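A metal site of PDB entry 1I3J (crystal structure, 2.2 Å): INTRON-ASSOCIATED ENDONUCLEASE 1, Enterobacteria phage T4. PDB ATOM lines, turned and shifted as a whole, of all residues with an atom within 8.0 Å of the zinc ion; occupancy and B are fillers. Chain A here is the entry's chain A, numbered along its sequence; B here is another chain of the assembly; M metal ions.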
ATOM      1  N   PHE A  21      15.819  -9.596 -24.211  1.00  0.00           N
ATOM      2  CA  PHE A  21      15.284  -9.792 -25.557  1.00  0.00           C
ATOM      3  C   PHE A  21      14.541 -11.115 -25.712  1.00  0.00           C
ATOM      4  O   PHE A  21      14.928 -12.142 -25.159  1.00  0.00           O
ATOM      5  CB  PHE A  21      16.392  -9.761 -26.608  1.00  0.00           C
ATOM      6  CG  PHE A  21      17.067  -8.434 -26.729  1.00  0.00           C
ATOM      7  CD1 PHE A  21      18.174  -8.125 -25.950  1.00  0.00           C
ATOM      8  CD2 PHE A  21      16.561  -7.484 -27.604  1.00  0.00           C
ATOM      9  CE1 PHE A  21      18.777  -6.880 -26.045  1.00  0.00           C
ATOM     10  CE2 PHE A  21      17.152  -6.234 -27.706  1.00  0.00           C
ATOM     11  CZ  PHE A  21      18.257  -5.932 -26.915  1.00  0.00           C
ATOM     12  N   CYS A  22      13.465 -11.073 -26.476  1.00  0.00           N
ATOM     13  CA  CYS A  22      12.684 -12.259 -26.755  1.00  0.00           C
ATOM     14  C   CYS A  22      13.443 -13.006 -27.853  1.00  0.00           C
ATOM     15  O   CYS A  22      14.258 -12.415 -28.582  1.00  0.00           O
ATOM     16  CB  CYS A  22      11.302 -11.854 -27.260  1.00  0.00           C
ATOM     17  SG  CYS A  22      10.269 -13.233 -27.830  1.00  0.00           S
ATOM     18  N   LYS A  23      13.169 -14.296 -27.995  1.00  0.00           N
ATOM     19  CA  LYS A  23      13.801 -15.112 -29.019  1.00  0.00           C
ATOM     20  C   LYS A  23      13.632 -14.474 -30.405  1.00  0.00           C
ATOM     21  O   LYS A  23      14.486 -14.617 -31.269  1.00  0.00           O
ATOM     22  CB  LYS A  23      13.205 -16.523 -29.042  1.00  0.00           C
ATOM     23  CG  LYS A  23      11.717 -16.559 -29.427  1.00  0.00           C
ATOM     24  CD  LYS A  23      11.084 -17.932 -29.261  1.00  0.00           C
ATOM     25  CE  LYS A  23      10.612 -18.220 -27.840  1.00  0.00           C
ATOM     26  NZ  LYS A  23      11.710 -18.337 -26.838  1.00  0.00           N
ATOM     27  N   CYS A  24      12.494 -13.782 -30.608  1.00  0.00           N
ATOM     28  CA  CYS A  24      12.179 -13.143 -31.891  1.00  0.00           C
ATOM     29  C   CYS A  24      13.020 -11.901 -32.153  1.00  0.00           C
ATOM     30  O   CYS A  24      13.116 -11.440 -33.287  1.00  0.00           O
ATOM     31  CB  CYS A  24      10.692 -12.759 -31.930  1.00  0.00           C
ATOM     32  SG  CYS A  24      10.262 -11.283 -30.929  1.00  0.00           S
ATOM     33  N   GLY A  25      13.612 -11.343 -31.102  1.00  0.00           N
ATOM     34  CA  GLY A  25      14.414 -10.150 -31.291  1.00  0.00           C
ATOM     35  C   GLY A  25      13.972  -8.870 -30.601  1.00  0.00           C
ATOM     36  O   GLY A  25      14.808  -7.995 -30.394  1.00  0.00           O
ATOM     37  N   VAL A  26      12.690  -8.734 -30.239  1.00  0.00           N
ATOM     38  CA  VAL A  26      12.241  -7.514 -29.559  1.00  0.00           C
ATOM     39  C   VAL A  26      12.636  -7.482 -28.088  1.00  0.00           C
ATOM     40  O   VAL A  26      13.032  -8.505 -27.506  1.00  0.00           O
ATOM     41  CB  VAL A  26      10.698  -7.297 -29.619  1.00  0.00           C
ATOM     42  CG1 VAL A  26      10.238  -7.270 -31.065  1.00  0.00           C
ATOM     43  CG2 VAL A  26       9.962  -8.373 -28.797  1.00  0.00           C
ATOM     44  N   ARG A  27      12.568  -6.285 -27.495  1.00  0.00           N
ATOM     45  CA  ARG A  27      12.871  -6.147 -26.082  1.00  0.00           C
ATOM     46  C   ARG A  27      11.642  -6.548 -25.258  1.00  0.00           C
ATOM     47  O   ARG A  27      10.504  -6.357 -25.690  1.00  0.00           O
ATOM     48  CB  ARG A  27      13.257  -4.710 -25.744  1.00  0.00           C
ATOM     49  CG  ARG A  27      14.454  -4.206 -26.529  1.00  0.00           C
ATOM     50  CD  ARG A  27      14.619  -2.716 -26.378  1.00  0.00           C
ATOM     51  NE  ARG A  27      15.921  -2.240 -26.822  1.00  0.00           N
ATOM     52  CZ  ARG A  27      16.367  -1.008 -26.626  1.00  0.00           C
ATOM     53  NH1 ARG A  27      15.611  -0.126 -25.974  1.00  0.00           N
ATOM     54  NH2 ARG A  27      17.564  -0.652 -27.070  1.00  0.00           N
ATOM     55  N   ILE A  28      11.882  -7.093 -24.079  1.00  0.00           N
ATOM     56  CA  ILE A  28      10.812  -7.509 -23.169  1.00  0.00           C
ATOM     57  C   ILE A  28      11.323  -7.249 -21.749  1.00  0.00           C
ATOM     58  O   ILE A  28      12.533  -7.094 -21.561  1.00  0.00           O
ATOM     59  CB  ILE A  28      10.470  -9.012 -23.310  1.00  0.00           C
ATOM     60  CG1 ILE A  28      11.744  -9.864 -23.164  1.00  0.00           C
ATOM     61  CG2 ILE A  28       9.812  -9.267 -24.648  1.00  0.00           C
ATOM     62  CD1 ILE A  28      11.494 -11.365 -23.284  1.00  0.00           C
ATOM     63  N   TYR A  33       9.148 -14.185 -20.217  1.00  0.00           N
ATOM     64  CA  TYR A  33       9.880 -15.270 -20.865  1.00  0.00           C
ATOM     65  C   TYR A  33       9.934 -15.043 -22.368  1.00  0.00           C
ATOM     66  O   TYR A  33      10.840 -15.534 -23.030  1.00  0.00           O
ATOM     67  CB  TYR A  33       9.216 -16.622 -20.584  1.00  0.00           C
ATOM     68  CG  TYR A  33       9.497 -17.183 -19.205  1.00  0.00           C
ATOM     69  CD1 TYR A  33       9.240 -16.422 -18.058  1.00  0.00           C
ATOM     70  CD2 TYR A  33       9.965 -18.489 -19.046  1.00  0.00           C
ATOM     71  CE1 TYR A  33       9.438 -16.958 -16.781  1.00  0.00           C
ATOM     72  CE2 TYR A  33      10.163 -19.040 -17.778  1.00  0.00           C
ATOM     73  CZ  TYR A  33       9.896 -18.268 -16.651  1.00  0.00           C
ATOM     74  OH  TYR A  33      10.088 -18.807 -15.393  1.00  0.00           O
ATOM     75  N   THR A  34       8.937 -14.344 -22.909  1.00  0.00           N
ATOM     76  CA  THR A  34       8.869 -14.033 -24.338  1.00  0.00           C
ATOM     77  C   THR A  34       8.014 -12.784 -24.515  1.00  0.00           C
ATOM     78  O   THR A  34       7.454 -12.260 -23.550  1.00  0.00           O
ATOM     79  CB  THR A  34       8.181 -15.133 -25.163  1.00  0.00           C
ATOM     80  OG1 THR A  34       6.755 -15.077 -24.964  1.00  0.00           O
ATOM     81  CG2 THR A  34       8.680 -16.514 -24.780  1.00  0.00           C
ATOM     82  N   CYS A  35       7.910 -12.326 -25.749  1.00  0.00           N
ATOM     83  CA  CYS A  35       7.079 -11.171 -26.017  1.00  0.00           C
ATOM     84  C   CYS A  35       5.682 -11.784 -26.065  1.00  0.00           C
ATOM     85  O   CYS A  35       5.533 -13.004 -26.142  1.00  0.00           O
ATOM     86  CB  CYS A  35       7.419 -10.539 -27.366  1.00  0.00           C
ATOM     87  SG  CYS A  35       6.950 -11.532 -28.773  1.00  0.00           S
ATOM     88  N   SER A  36       4.653 -10.944 -26.039  1.00  0.00           N
ATOM     89  CA  SER A  36       3.292 -11.448 -26.094  1.00  0.00           C
ATOM     90  C   SER A  36       2.997 -12.274 -27.350  1.00  0.00           C
ATOM     91  O   SER A  36       2.316 -13.293 -27.291  1.00  0.00           O
ATOM     92  CB  SER A  36       2.304 -10.304 -26.028  1.00  0.00           C
ATOM     93  OG  SER A  36       0.991 -10.826 -26.086  1.00  0.00           O
ATOM     94  N   LYS A  37       3.512 -11.829 -28.487  1.00  0.00           N
ATOM     95  CA  LYS A  37       3.272 -12.539 -29.736  1.00  0.00           C
ATOM     96  C   LYS A  37       3.878 -13.933 -29.773  1.00  0.00           C
ATOM     97  O   LYS A  37       3.263 -14.859 -30.284  1.00  0.00           O
ATOM     98  CB  LYS A  37       3.815 -11.711 -30.905  1.00  0.00           C
ATOM     99  CG  LYS A  37       3.369 -12.208 -32.271  1.00  0.00           C
ATOM    100  CD  LYS A  37       1.882 -11.939 -32.540  1.00  0.00           C
ATOM    101  CE  LYS A  37       1.455 -12.518 -33.902  1.00  0.00           C
ATOM    102  NZ  LYS A  37       0.102 -12.076 -34.390  1.00  0.00           N
ATOM    103  N   CYS A  38       5.066 -14.089 -29.192  1.00  0.00           N
ATOM    104  CA  CYS A  38       5.767 -15.377 -29.181  1.00  0.00           C
ATOM    105  C   CYS A  38       5.376 -16.386 -28.103  1.00  0.00           C
ATOM    106  O   CYS A  38       5.861 -17.515 -28.103  1.00  0.00           O
ATOM    107  CB  CYS A  38       7.285 -15.141 -29.111  1.00  0.00           C
ATOM    108  SG  CYS A  38       7.947 -14.135 -30.474  1.00  0.00           S
ATOM    109  N   ARG A  39       4.511 -15.993 -27.164  1.00  0.00           N
ATOM    110  CA  ARG A  39       4.093 -16.907 -26.101  1.00  0.00           C
ATOM    111  C   ARG A  39       3.374 -18.124 -26.685  1.00  0.00           C
ATOM    112  O   ARG A  39       2.507 -17.988 -27.556  1.00  0.00           O
ATOM    113  CB  ARG A  39       3.187 -16.179 -25.098  1.00  0.00           C
ATOM    114  CG  ARG A  39       2.630 -17.050 -23.971  1.00  0.00           C
ATOM    115  CD  ARG A  39       1.742 -16.240 -23.017  1.00  0.00           C
ATOM    116  NE  ARG A  39       1.028 -17.084 -22.043  1.00  0.00           N
ATOM    117  CZ  ARG A  39       0.024 -16.676 -21.260  1.00  0.00           C
ATOM    118  NH1 ARG A  39      -0.416 -15.422 -21.314  1.00  0.00           N
ATOM    119  NH2 ARG A  39      -0.587 -17.526 -20.449  1.00  0.00           N
ATOM    120  P    DA B  21       5.314  -8.107 -23.856  1.00  0.00           P
ATOM    121  OP1  DA B  21       5.436  -8.191 -25.339  1.00  0.00           O
ATOM    122  OP2  DA B  21       6.537  -8.124 -23.019  1.00  0.00           O
ATOM    123  O5'  DA B  21       4.477  -6.803 -23.523  1.00  0.00           O
ATOM    124  C5'  DA B  21       3.364  -6.882 -22.656  1.00  0.00           C
ATOM    125  C4'  DA B  21       2.675  -5.556 -22.570  1.00  0.00           C
ATOM    126  O4'  DA B  21       1.767  -5.630 -21.443  1.00  0.00           O
ATOM    127  C3'  DA B  21       3.644  -4.424 -22.231  1.00  0.00           C
ATOM    128  O3'  DA B  21       3.033  -3.209 -22.616  1.00  0.00           O
ATOM    129  C2'  DA B  21       3.696  -4.479 -20.715  1.00  0.00           C
ATOM    130  C1'  DA B  21       2.267  -4.874 -20.356  1.00  0.00           C
ATOM    131  N9   DA B  21       2.158  -5.676 -19.149  1.00  0.00           N
ATOM    132  C8   DA B  21       3.048  -6.593 -18.647  1.00  0.00           C
ATOM    133  N7   DA B  21       2.677  -7.119 -17.504  1.00  0.00           N
ATOM    134  C5   DA B  21       1.447  -6.533 -17.255  1.00  0.00           C
ATOM    135  C6   DA B  21       0.534  -6.663 -16.194  1.00  0.00           C
ATOM    136  N6   DA B  21       0.723  -7.476 -15.142  1.00  0.00           N
ATOM    137  N1   DA B  21      -0.596  -5.924 -16.246  1.00  0.00           N
ATOM    138  C2   DA B  21      -0.781  -5.110 -17.289  1.00  0.00           C
ATOM    139  N3   DA B  21       0.008  -4.893 -18.341  1.00  0.00           N
ATOM    140  C4   DA B  21       1.114  -5.643 -18.257  1.00  0.00           C
HETATM  141 ZN    ZN M   1       8.897 -12.536 -29.405  1.00  0.00          ZN
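The side-chain sulfur (SG) of Cys 35 lies close to the backbone NH (N) of Lys 37 (3.5 Å). SG of Cys 24 sits close to N of Val 26, at 3.6 Å.
Four residues have an atom within 4 Å of the zinc ion: Cys 22, Cys 24, Cys 35 and Cys 38.
The zinc ion is bound by the side-chain sulfur of Cys 38 (2.1 Å), the side-chain sulfur of Cys 22 (2.2 Å), the side-chain sulfur of Cys 35 (2.3 Å) and the side-chain sulfur of Cys 24 (2.4 Å). The zinc ion has four donor atoms within binding distance.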
